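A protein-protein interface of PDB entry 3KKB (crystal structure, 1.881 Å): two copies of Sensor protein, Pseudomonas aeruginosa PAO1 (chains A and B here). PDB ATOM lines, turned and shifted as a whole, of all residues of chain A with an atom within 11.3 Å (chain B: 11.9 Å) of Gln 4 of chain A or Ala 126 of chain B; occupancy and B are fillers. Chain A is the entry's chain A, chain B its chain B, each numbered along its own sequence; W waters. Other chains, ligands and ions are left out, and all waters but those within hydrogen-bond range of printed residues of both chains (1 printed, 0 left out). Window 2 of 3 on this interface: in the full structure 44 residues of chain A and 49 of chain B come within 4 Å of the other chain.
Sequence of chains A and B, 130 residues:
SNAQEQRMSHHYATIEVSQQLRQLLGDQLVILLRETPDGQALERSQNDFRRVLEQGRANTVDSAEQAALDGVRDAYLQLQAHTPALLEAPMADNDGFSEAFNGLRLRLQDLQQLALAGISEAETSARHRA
OH of Tyr 12 of chain A lies within hydrogen-bond range of OE2 of Glu 123 of chain A, at 3.3 Å.
Gln 4 of chain A touches Ala 126 of chain B (OE1 to CB, 3.9 Å). Ile 119 of chain B touches Met 8 of chain A (O to CE, 3.5 Å). Glu 123 of chain B touches Met 8 of chain A. O of Gly 118 of chain B touches CD2 of His 11 of chain A (3.9 Å). His 11 of chain A touches Ile 119 of chain B (CB to CG1, 3.7 Å). Tyr 12 of chain A touches Ile 119 of chain B (OH to CG2, 3.5 Å). Ala 122 of chain A touches Gln 4 of chain B. Ala 122 of chain A touches Met 8 of chain B. Glu 123 of chain A touches Met 8 of chain B. CG of Glu 123 of chain A touches OE1 of Glu 123 of chain B (2.8 Å).
Gln 4 of chain A touches just one residue of chain B: Ala 126. Ala 126 of chain B touches one residue of chain A. No residue of chain B comes within 4 Å of Ser 1 of chain A. No residue of chain B comes within 4 Å of Ala 3 of chain A. No residue of chain B comes within 4 Å of Gln 6 of chain A. No residue of chain B comes within 4 Å of Arg 7 of chain A. Of chain B, only Ile 119 (3.5 Å), Ala 122 (3.5 Å) and Glu 123 (3.3 Å) come within 4 Å of Met 8 of chain A. No residue of chain A comes within 4 Å of Thr 124 of chain B. No residue of chain A comes within 4 Å of Ser 125 of chain B. No residue of chain A comes within 4 Å of His 128 of chain B. Printed residues of chain B within 4 Å of His 11 of chain A: Gly 118 and Ile 119. Of the printed residues of chain B, Tyr 12 of chain A touches Ile 119. The nearest residue of chain B that does not touch Gln 4 of chain A is Ser 125 of chain B (5.4 Å). The nearest printed residue of chain A that does not touch Met 8 of chain B is Ala 126 of chain A (6.0 Å).
Hydrophobic or aromatic side chains of chain B that line the printed part of chain A: Met 8, Ile 119, Ala 122 and Ala 126. Of the 19 printed residues of chain A, 6 touch a printed residue of chain B. Hydrophobic or aromatic side chains of chain A within 4 Å of the printed part of chain B: Met 8, His 11, Tyr 12 and Ala 122. Among the printed residues, 11 pairs touch across the chains. Among the printed residues, no Asp or Glu carboxylate lies within 4 Å of a Lys or Arg side-chain nitrogen of the other chain.
Gln 4 of chain A touches Ala 126 of chain B, but with the chains exchanged Ala 126 of chain A does not touch Gln 4 of chain B (5.1 Å). Met 8 of chain A touches Ala 122 of chain B, and with the chains exchanged Ala 122 of chain A touches Met 8 of chain B. Ala 122 of chain A touches Gln 4 of chain B, but with the chains exchanged Gln 4 of chain A does not touch Ala 122 of chain B (5.6 Å). Glu 123 of chain B touches its own counterpart, Glu 123 of chain A. Positions printed for both chains: 4, 8, 12, 122, 123, 124, 125 and 126. Of the 11 pairs that touch across the chains among the printed residues, 5 have their exchanged pair printed and touching as well.
Water W1 lies within hydrogen-bond range of the backbone carbonyl oxygen of Gly 118 of chain B (2.9 Å) and a ring nitrogen (NE2) of His 11 of chain A (3.4 Å).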
ATOM      1  N   SER A   1     -30.785  16.453  -4.786  1.00  0.00           N
ATOM      2  CA  SER A   1     -31.348  17.097  -5.966  1.00  0.00           C
ATOM      3  C   SER A   1     -31.563  18.588  -5.734  1.00  0.00           C
ATOM      4  O   SER A   1     -31.607  19.370  -6.683  1.00  0.00           O
ATOM      5  CB  SER A   1     -32.665  16.429  -6.370  1.00  0.00           C
ATOM      6  OG  SER A   1     -33.588  16.421  -5.293  1.00  0.00           O
ATOM      7  N   ASN A   2     -31.703  18.976  -4.470  1.00  0.00           N
ATOM      8  CA  ASN A   2     -31.849  20.385  -4.126  1.00  0.00           C
ATOM      9  C   ASN A   2     -30.521  21.113  -4.284  1.00  0.00           C
ATOM     10  O   ASN A   2     -30.472  22.232  -4.790  1.00  0.00           O
ATOM     11  CB  ASN A   2     -32.381  20.550  -2.702  1.00  0.00           C
ATOM     12  CG  ASN A   2     -32.889  21.954  -2.429  1.00  0.00           C
ATOM     13  OD1 ASN A   2     -33.422  22.618  -3.320  1.00  0.00           O
ATOM     14  ND2 ASN A   2     -32.733  22.412  -1.192  1.00  0.00           N
ATOM     15  N   ALA A   3     -29.445  20.462  -3.853  1.00  0.00           N
ATOM     16  CA  ALA A   3     -28.108  21.009  -4.023  1.00  0.00           C
ATOM     17  C   ALA A   3     -27.823  21.246  -5.501  1.00  0.00           C
ATOM     18  O   ALA A   3     -27.091  22.161  -5.865  1.00  0.00           O
ATOM     19  CB  ALA A   3     -27.077  20.074  -3.429  1.00  0.00           C
ATOM     20  N   GLN A   4     -28.411  20.408  -6.347  1.00  0.00           N
ATOM     21  CA  GLN A   4     -28.253  20.521  -7.790  1.00  0.00           C
ATOM     22  C   GLN A   4     -28.933  21.789  -8.303  1.00  0.00           C
ATOM     23  O   GLN A   4     -28.344  22.566  -9.060  1.00  0.00           O
ATOM     24  CB  GLN A   4     -28.851  19.284  -8.461  1.00  0.00           C
ATOM     25  CG  GLN A   4     -28.594  19.161  -9.949  1.00  0.00           C
ATOM     26  CD  GLN A   4     -29.209  17.897 -10.531  1.00  0.00           C
ATOM     27  OE1 GLN A   4     -28.737  17.365 -11.537  1.00  0.00           O
ATOM     28  NE2 GLN A   4     -30.267  17.404  -9.889  1.00  0.00           N
ATOM     29  N   GLU A   5     -30.175  21.998  -7.880  1.00  0.00           N
ATOM     30  CA  GLU A   5     -30.934  23.170  -8.305  1.00  0.00           C
ATOM     31  C   GLU A   5     -30.389  24.459  -7.689  1.00  0.00           C
ATOM     32  O   GLU A   5     -30.517  25.534  -8.276  1.00  0.00           O
ATOM     33  CB  GLU A   5     -32.419  23.000  -7.979  1.00  0.00           C
ATOM     34  CG  GLU A   5     -33.012  21.702  -8.517  1.00  0.00           C
ATOM     35  CD  GLU A   5     -34.525  21.745  -8.629  1.00  0.00           C
ATOM     36  OE1 GLU A   5     -35.067  22.797  -9.034  1.00  0.00           O
ATOM     37  OE2 GLU A   5     -35.171  20.719  -8.322  1.00  0.00           O
ATOM     38  N   GLN A   6     -29.778  24.341  -6.512  1.00  0.00           N
ATOM     39  CA  GLN A   6     -29.157  25.484  -5.844  1.00  0.00           C
ATOM     40  C   GLN A   6     -27.862  25.919  -6.531  1.00  0.00           C
ATOM     41  O   GLN A   6     -27.583  27.111  -6.635  1.00  0.00           O
ATOM     42  CB  GLN A   6     -28.896  25.187  -4.364  1.00  0.00           C
ATOM     43  CG  GLN A   6     -30.157  25.083  -3.523  1.00  0.00           C
ATOM     44  CD  GLN A   6     -31.107  26.247  -3.749  1.00  0.00           C
ATOM     45  OE1 GLN A   6     -30.900  27.344  -3.227  1.00  0.00           O
ATOM     46  NE2 GLN A   6     -32.157  26.010  -4.528  1.00  0.00           N
ATOM     47  N   ARG A   7     -27.071  24.957  -6.991  1.00  0.00           N
ATOM     48  CA  ARG A   7     -25.863  25.269  -7.752  1.00  0.00           C
ATOM     49  C   ARG A   7     -26.227  25.965  -9.059  1.00  0.00           C
ATOM     50  O   ARG A   7     -25.563  26.917  -9.482  1.00  0.00           O
ATOM     51  CB  ARG A   7     -25.054  24.002  -8.038  1.00  0.00           C
ATOM     52  CG  ARG A   7     -24.083  23.614  -6.924  1.00  0.00           C
ATOM     53  CD  ARG A   7     -24.175  22.132  -6.573  1.00  0.00           C
ATOM     54  NE  ARG A   7     -23.970  21.257  -7.726  1.00  0.00           N
ATOM     55  CZ  ARG A   7     -24.027  19.929  -7.672  1.00  0.00           C
ATOM     56  NH1 ARG A   7     -23.829  19.206  -8.766  1.00  0.00           N
ATOM     57  NH2 ARG A   7     -24.284  19.323  -6.520  1.00  0.00           N
ATOM     58  N   MET A   8     -27.283  25.480  -9.699  1.00  0.00           N
ATOM     59  CA  MET A   8     -27.784  26.096 -10.923  1.00  0.00           C
ATOM     60  C   MET A   8     -28.263  27.524 -10.666  1.00  0.00           C
ATOM     61  O   MET A   8     -27.929  28.457 -11.402  1.00  0.00           O
ATOM     62  CB  MET A   8     -28.935  25.272 -11.498  1.00  0.00           C
ATOM     63  CG  MET A   8     -29.608  25.945 -12.669  1.00  0.00           C
ATOM     64  SD  MET A   8     -28.316  26.280 -14.101  1.00  0.00           S
ATOM     65  CE  MET A   8     -28.415  24.542 -14.980  1.00  0.00           C
ATOM     66  N   SER A   9     -29.057  27.682  -9.614  1.00  0.00           N
ATOM     67  CA  SER A   9     -29.570  28.984  -9.224  1.00  0.00           C
ATOM     68  C   SER A   9     -28.445  29.989  -8.930  1.00  0.00           C
ATOM     69  O   SER A   9     -28.553  31.170  -9.260  1.00  0.00           O
ATOM     70  CB  SER A   9     -30.488  28.841  -8.008  1.00  0.00           C
ATOM     71  OG  SER A   9     -31.040  30.094  -7.647  1.00  0.00           O
ATOM     72  N   HIS A  10     -27.366  29.523  -8.314  1.00  0.00           N
ATOM     73  CA  HIS A  10     -26.250  30.412  -7.997  1.00  0.00           C
ATOM     74  C   HIS A  10     -25.506  30.875  -9.245  1.00  0.00           C
ATOM     75  O   HIS A  10     -24.985  31.992  -9.289  1.00  0.00           O
ATOM     76  CB  HIS A  10     -25.289  29.751  -7.007  1.00  0.00           C
ATOM     77  CG  HIS A  10     -25.716  29.898  -5.582  1.00  0.00           C
ATOM     78  ND1 HIS A  10     -26.155  28.837  -4.821  1.00  0.00           N
ATOM     79  CD2 HIS A  10     -25.792  30.990  -4.786  1.00  0.00           C
ATOM     80  CE1 HIS A  10     -26.473  29.267  -3.612  1.00  0.00           C
ATOM     81  NE2 HIS A  10     -26.261  30.570  -3.565  1.00  0.00           N
ATOM     82  N   HIS A  11     -25.450  30.019 -10.263  1.00  0.00           N
ATOM     83  CA  HIS A  11     -24.895  30.441 -11.552  1.00  0.00           C
ATOM     84  C   HIS A  11     -25.729  31.564 -12.175  1.00  0.00           C
ATOM     85  O   HIS A  11     -25.179  32.556 -12.653  1.00  0.00           O
ATOM     86  CB  HIS A  11     -24.777  29.264 -12.529  1.00  0.00           C
ATOM     87  CG  HIS A  11     -23.744  28.249 -12.143  1.00  0.00           C
ATOM     88  ND1 HIS A  11     -22.426  28.579 -11.898  1.00  0.00           N
ATOM     89  CD2 HIS A  11     -23.827  26.908 -11.980  1.00  0.00           C
ATOM     90  CE1 HIS A  11     -21.748  27.490 -11.590  1.00  0.00           C
ATOM     91  NE2 HIS A  11     -22.576  26.458 -11.633  1.00  0.00           N
ATOM     92  N   TYR A  12     -27.052  31.404 -12.201  1.00  0.00           N
ATOM     93  CA  TYR A  12     -27.909  32.487 -12.701  1.00  0.00           C
ATOM     94  C   TYR A  12     -27.725  33.770 -11.900  1.00  0.00           C
ATOM     95  O   TYR A  12     -27.661  34.860 -12.466  1.00  0.00           O
ATOM     96  CB  TYR A  12     -29.390  32.080 -12.717  1.00  0.00           C
ATOM     97  CG  TYR A  12     -29.785  31.230 -13.910  1.00  0.00           C
ATOM     98  CD1 TYR A  12     -29.963  31.796 -15.171  1.00  0.00           C
ATOM     99  CD2 TYR A  12     -29.969  29.865 -13.776  1.00  0.00           C
ATOM    100  CE1 TYR A  12     -30.318  31.005 -16.265  1.00  0.00           C
ATOM    101  CE2 TYR A  12     -30.326  29.075 -14.856  1.00  0.00           C
ATOM    102  CZ  TYR A  12     -30.498  29.647 -16.095  1.00  0.00           C
ATOM    103  OH  TYR A  12     -30.860  28.842 -17.157  1.00  0.00           O
ATOM    104  N   ALA A  13     -27.652  33.650 -10.580  1.00  0.00           N
ATOM    105  CA  ALA A  13     -27.453  34.825  -9.737  1.00  0.00           C
ATOM    106  C   ALA A  13     -26.192  35.550 -10.167  1.00  0.00           C
ATOM    107  O   ALA A  13     -26.162  36.769 -10.264  1.00  0.00           O
ATOM    108  CB  ALA A  13     -27.353  34.420  -8.266  1.00  0.00           C
ATOM    109  N   ASP A  62     -19.473  29.251  -5.507  1.00  0.00           N
ATOM    110  CA  ASP A  62     -18.593  28.660  -6.505  1.00  0.00           C
ATOM    111  C   ASP A  62     -17.206  29.299  -6.461  1.00  0.00           C
ATOM    112  O   ASP A  62     -17.090  30.518  -6.487  1.00  0.00           O
ATOM    113  CB  ASP A  62     -19.210  28.808  -7.894  1.00  0.00           C
ATOM    114  CG  ASP A  62     -18.377  28.157  -8.970  1.00  0.00           C
ATOM    115  OD1 ASP A  62     -18.512  26.940  -9.176  1.00  0.00           O
ATOM    116  OD2 ASP A  62     -17.587  28.859  -9.617  1.00  0.00           O
ATOM    117  N   ALA A 122     -35.892  28.017 -21.823  1.00  0.00           N
ATOM    118  CA  ALA A 122     -35.546  26.709 -22.364  1.00  0.00           C
ATOM    119  C   ALA A 122     -34.991  25.757 -21.293  1.00  0.00           C
ATOM    120  O   ALA A 122     -35.263  24.555 -21.322  1.00  0.00           O
ATOM    121  CB  ALA A 122     -34.570  26.865 -23.525  1.00  0.00           C
ATOM    122  N   GLU A 123     -34.226  26.299 -20.348  1.00  0.00           N
ATOM    123  CA  GLU A 123     -33.676  25.523 -19.233  1.00  0.00           C
ATOM    124  C   GLU A 123     -34.762  25.085 -18.250  1.00  0.00           C
ATOM    125  O   GLU A 123     -34.891  23.901 -17.942  1.00  0.00           O
ATOM    126  CB  GLU A 123     -32.607  26.336 -18.489  1.00  0.00           C
ATOM    127  CG  GLU A 123     -31.918  25.598 -17.336  1.00  0.00           C
ATOM    128  CD  GLU A 123     -32.565  25.835 -15.977  1.00  0.00           C
ATOM    129  OE1 GLU A 123     -32.477  24.932 -15.116  1.00  0.00           O
ATOM    130  OE2 GLU A 123     -33.143  26.921 -15.757  1.00  0.00           O
ATOM    131  N   THR A 124     -35.537  26.050 -17.762  1.00  0.00           N
ATOM    132  CA  THR A 124     -36.582  25.784 -16.773  1.00  0.00           C
ATOM    133  C   THR A 124     -37.671  24.859 -17.319  1.00  0.00           C
ATOM    134  O   THR A 124     -38.181  23.997 -16.601  1.00  0.00           O
ATOM    135  CB  THR A 124     -37.233  27.088 -16.264  1.00  0.00           C
ATOM    136  OG1 THR A 124     -37.889  27.756 -17.348  1.00  0.00           O
ATOM    137  CG2 THR A 124     -36.182  28.013 -15.665  1.00  0.00           C
ATOM    138  N   SER A 125     -38.022  25.045 -18.588  1.00  0.00           N
ATOM    139  CA  SER A 125     -39.011  24.198 -19.248  1.00  0.00           C
ATOM    140  C   SER A 125     -38.509  22.762 -19.368  1.00  0.00           C
ATOM    141  O   SER A 125     -39.244  21.868 -19.789  1.00  0.00           O
ATOM    142  CB  SER A 125     -39.357  24.750 -20.635  1.00  0.00           C
ATOM    143  OG  SER A 125     -39.994  26.015 -20.546  1.00  0.00           O
ATOM    144  N   ALA A 126     -37.250  22.551 -18.995  1.00  0.00           N
ATOM    145  CA  ALA A 126     -36.664  21.218 -18.998  1.00  0.00           C
ATOM    146  C   ALA A 126     -35.565  21.103 -17.948  1.00  0.00           C
ATOM    147  O   ALA A 126     -35.841  20.866 -16.762  1.00  0.00           O
ATOM    148  CB  ALA A 126     -36.116  20.888 -20.379  1.00  0.00           C
ATOM    149  N   GLN B   4     -36.970  22.168 -29.251  1.00  0.00           N
ATOM    150  CA  GLN B   4     -36.433  22.717 -28.009  1.00  0.00           C
ATOM    151  C   GLN B   4     -34.958  23.094 -28.144  1.00  0.00           C
ATOM    152  O   GLN B   4     -34.546  24.187 -27.752  1.00  0.00           O
ATOM    153  CB  GLN B   4     -36.609  21.720 -26.861  1.00  0.00           C
ATOM    154  CG  GLN B   4     -36.591  22.346 -25.467  1.00  0.00           C
ATOM    155  CD  GLN B   4     -35.308  23.105 -25.170  1.00  0.00           C
ATOM    156  OE1 GLN B   4     -35.286  24.337 -25.162  1.00  0.00           O
ATOM    157  NE2 GLN B   4     -34.231  22.370 -24.923  1.00  0.00           N
ATOM    158  N   MET B   8     -33.233  26.880 -28.002  1.00  0.00           N
ATOM    159  CA  MET B   8     -32.123  27.068 -27.075  1.00  0.00           C
ATOM    160  C   MET B   8     -30.859  27.517 -27.816  1.00  0.00           C
ATOM    161  O   MET B   8     -30.109  28.366 -27.340  1.00  0.00           O
ATOM    162  CB  MET B   8     -31.842  25.763 -26.336  1.00  0.00           C
ATOM    163  CG  MET B   8     -30.683  25.848 -25.363  1.00  0.00           C
ATOM    164  SD  MET B   8     -31.296  26.236 -23.561  1.00  0.00           S
ATOM    165  CE  MET B   8     -32.317  24.601 -23.263  1.00  0.00           C
ATOM    166  N   TYR B  12     -28.579  31.045 -27.576  1.00  0.00           N
ATOM    167  CA  TYR B  12     -27.123  31.049 -27.380  1.00  0.00           C
ATOM    168  C   TYR B  12     -26.402  31.767 -28.508  1.00  0.00           C
ATOM    169  O   TYR B  12     -25.402  32.443 -28.282  1.00  0.00           O
ATOM    170  CB  TYR B  12     -26.562  29.631 -27.218  1.00  0.00           C
ATOM    171  CG  TYR B  12     -26.664  29.129 -25.803  1.00  0.00           C
ATOM    172  CD1 TYR B  12     -25.749  29.532 -24.843  1.00  0.00           C
ATOM    173  CD2 TYR B  12     -27.685  28.270 -25.419  1.00  0.00           C
ATOM    174  CE1 TYR B  12     -25.844  29.096 -23.540  1.00  0.00           C
ATOM    175  CE2 TYR B  12     -27.785  27.821 -24.116  1.00  0.00           C
ATOM    176  CZ  TYR B  12     -26.859  28.241 -23.182  1.00  0.00           C
ATOM    177  OH  TYR B  12     -26.943  27.800 -21.885  1.00  0.00           O
ATOM    178  N   ALA B 117     -21.048  29.757 -19.054  1.00  0.00           N
ATOM    179  CA  ALA B 117     -20.472  28.432 -19.253  1.00  0.00           C
ATOM    180  C   ALA B 117     -20.892  27.506 -18.121  1.00  0.00           C
ATOM    181  O   ALA B 117     -21.135  26.323 -18.344  1.00  0.00           O
ATOM    182  CB  ALA B 117     -18.954  28.520 -19.337  1.00  0.00           C
ATOM    183  N   GLY B 118     -20.980  28.048 -16.907  1.00  0.00           N
ATOM    184  CA  GLY B 118     -21.453  27.279 -15.762  1.00  0.00           C
ATOM    185  C   GLY B 118     -22.912  26.865 -15.906  1.00  0.00           C
ATOM    186  O   GLY B 118     -23.263  25.725 -15.646  1.00  0.00           O
ATOM    187  N   ILE B 119     -23.765  27.793 -16.327  1.00  0.00           N
ATOM    188  CA  ILE B 119     -25.178  27.480 -16.565  1.00  0.00           C
ATOM    189  C   ILE B 119     -25.326  26.347 -17.587  1.00  0.00           C
ATOM    190  O   ILE B 119     -25.992  25.343 -17.322  1.00  0.00           O
ATOM    191  CB  ILE B 119     -25.982  28.724 -17.039  1.00  0.00           C
ATOM    192  CG1 ILE B 119     -26.093  29.753 -15.904  1.00  0.00           C
ATOM    193  CG2 ILE B 119     -27.383  28.309 -17.466  1.00  0.00           C
ATOM    194  CD1 ILE B 119     -26.570  31.144 -16.354  1.00  0.00           C
ATOM    195  N   SER B 120     -24.682  26.494 -18.743  1.00  0.00           N
ATOM    196  CA  SER B 120     -24.789  25.490 -19.798  1.00  0.00           C
ATOM    197  C   SER B 120     -24.239  24.140 -19.367  1.00  0.00           C
ATOM    198  O   SER B 120     -24.802  23.097 -19.692  1.00  0.00           O
ATOM    199  CB  SER B 120     -24.057  25.950 -21.053  1.00  0.00           C
ATOM    200  OG  SER B 120     -24.412  27.277 -21.361  1.00  0.00           O
ATOM    201  N   GLU B 121     -23.125  24.157 -18.642  1.00  0.00           N
ATOM    202  CA  GLU B 121     -22.508  22.901 -18.233  1.00  0.00           C
ATOM    203  C   GLU B 121     -23.425  22.141 -17.279  1.00  0.00           C
ATOM    204  O   GLU B 121     -23.595  20.921 -17.392  1.00  0.00           O
ATOM    205  CB  GLU B 121     -21.125  23.156 -17.593  1.00  0.00           C
ATOM    206  CG  GLU B 121     -20.280  21.894 -17.437  1.00  0.00           C
ATOM    207  CD  GLU B 121     -19.595  21.469 -18.728  1.00  0.00           C
ATOM    208  OE1 GLU B 121     -19.371  20.254 -18.910  1.00  0.00           O
ATOM    209  OE2 GLU B 121     -19.264  22.350 -19.555  1.00  0.00           O
ATOM    210  N   ALA B 122     -24.036  22.870 -16.346  1.00  0.00           N
ATOM    211  CA  ALA B 122     -24.920  22.260 -15.356  1.00  0.00           C
ATOM    212  C   ALA B 122     -26.200  21.717 -15.988  1.00  0.00           C
ATOM    213  O   ALA B 122     -26.672  20.648 -15.632  1.00  0.00           O
ATOM    214  CB  ALA B 122     -25.263  23.254 -14.261  1.00  0.00           C
ATOM    215  N   GLU B 123     -26.768  22.468 -16.921  1.00  0.00           N
ATOM    216  CA  GLU B 123     -27.947  21.998 -17.630  1.00  0.00           C
ATOM    217  C   GLU B 123     -27.641  20.734 -18.430  1.00  0.00           C
ATOM    218  O   GLU B 123     -28.447  19.800 -18.474  1.00  0.00           O
ATOM    219  CB  GLU B 123     -28.480  23.083 -18.561  1.00  0.00           C
ATOM    220  CG  GLU B 123     -29.152  22.530 -19.801  1.00  0.00           C
ATOM    221  CD  GLU B 123     -30.205  23.459 -20.349  1.00  0.00           C
ATOM    222  OE1 GLU B 123     -30.784  24.227 -19.558  1.00  0.00           O
ATOM    223  OE2 GLU B 123     -30.459  23.414 -21.568  1.00  0.00           O
ATOM    224  N   THR B 124     -26.477  20.705 -19.064  1.00  0.00           N
ATOM    225  CA  THR B 124     -26.081  19.531 -19.840  1.00  0.00           C
ATOM    226  C   THR B 124     -25.826  18.338 -18.934  1.00  0.00           C
ATOM    227  O   THR B 124     -26.188  17.211 -19.259  1.00  0.00           O
ATOM    228  CB  THR B 124     -24.828  19.792 -20.710  1.00  0.00           C
ATOM    229  OG1 THR B 124     -25.088  20.873 -21.614  1.00  0.00           O
ATOM    230  CG2 THR B 124     -24.476  18.534 -21.514  1.00  0.00           C
ATOM    231  N   SER B 125     -25.191  18.580 -17.795  1.00  0.00           N
ATOM    232  CA  SER B 125     -24.927  17.495 -16.862  1.00  0.00           C
ATOM    233  C   SER B 125     -26.238  16.921 -16.317  1.00  0.00           C
ATOM    234  O   SER B 125     -26.361  15.716 -16.128  1.00  0.00           O
ATOM    235  CB  SER B 125     -24.030  17.973 -15.717  1.00  0.00           C
ATOM    236  OG  SER B 125     -23.756  16.919 -14.803  1.00  0.00           O
ATOM    237  N   ALA B 126     -27.214  17.793 -16.081  1.00  0.00           N
ATOM    238  CA  ALA B 126     -28.500  17.384 -15.525  1.00  0.00           C
ATOM    239  C   ALA B 126     -29.257  16.441 -16.459  1.00  0.00           C
ATOM    240  O   ALA B 126     -30.050  15.615 -16.000  1.00  0.00           O
ATOM    241  CB  ALA B 126     -29.350  18.606 -15.181  1.00  0.00           C
ATOM    242  N   ARG B 127     -29.010  16.561 -17.764  1.00  0.00           N
ATOM    243  CA  ARG B 127     -29.642  15.683 -18.754  1.00  0.00           C
ATOM    244  C   ARG B 127     -29.294  14.213 -18.518  1.00  0.00           C
ATOM    245  O   ARG B 127     -29.783  13.331 -19.219  1.00  0.00           O
ATOM    246  CB  ARG B 127     -29.236  16.069 -20.178  1.00  0.00           C
ATOM    247  CG  ARG B 127     -29.625  17.480 -20.619  1.00  0.00           C
ATOM    248  CD  ARG B 127     -29.411  17.641 -22.123  1.00  0.00           C
ATOM    249  NE  ARG B 127     -28.767  18.905 -22.485  1.00  0.00           N
ATOM    250  CZ  ARG B 127     -27.969  19.056 -23.540  1.00  0.00           C
ATOM    251  NH1 ARG B 127     -27.418  20.237 -23.805  1.00  0.00           N
ATOM    252  NH2 ARG B 127     -27.715  18.019 -24.329  1.00  0.00           N
ATOM    253  N   HIS B 128     -28.439  13.955 -17.536  1.00  0.00           N
ATOM    254  CA  HIS B 128     -28.080  12.588 -17.170  1.00  0.00           C
ATOM    255  C   HIS B 128     -28.649  12.229 -15.797  1.00  0.00           C
ATOM    256  O   HIS B 128     -29.862  12.078 -15.633  1.00  0.00           O
ATOM    257  CB  HIS B 128     -26.559  12.407 -17.178  1.00  0.00           C
ATOM    258  CG  HIS B 128     -25.910  12.827 -18.455  1.00  0.00           C
ATOM    259  ND1 HIS B 128     -25.740  11.971 -19.525  1.00  0.00           N
ATOM    260  CD2 HIS B 128     -25.380  14.013 -18.839  1.00  0.00           C
ATOM    261  CE1 HIS B 128     -25.141  12.613 -20.509  1.00  0.00           C
ATOM    262  NE2 HIS B 128     -24.911  13.856 -20.119  1.00  0.00           N
HETATM  263  O   HOH W   1     -21.570  24.131 -13.838  1.00  0.00           O
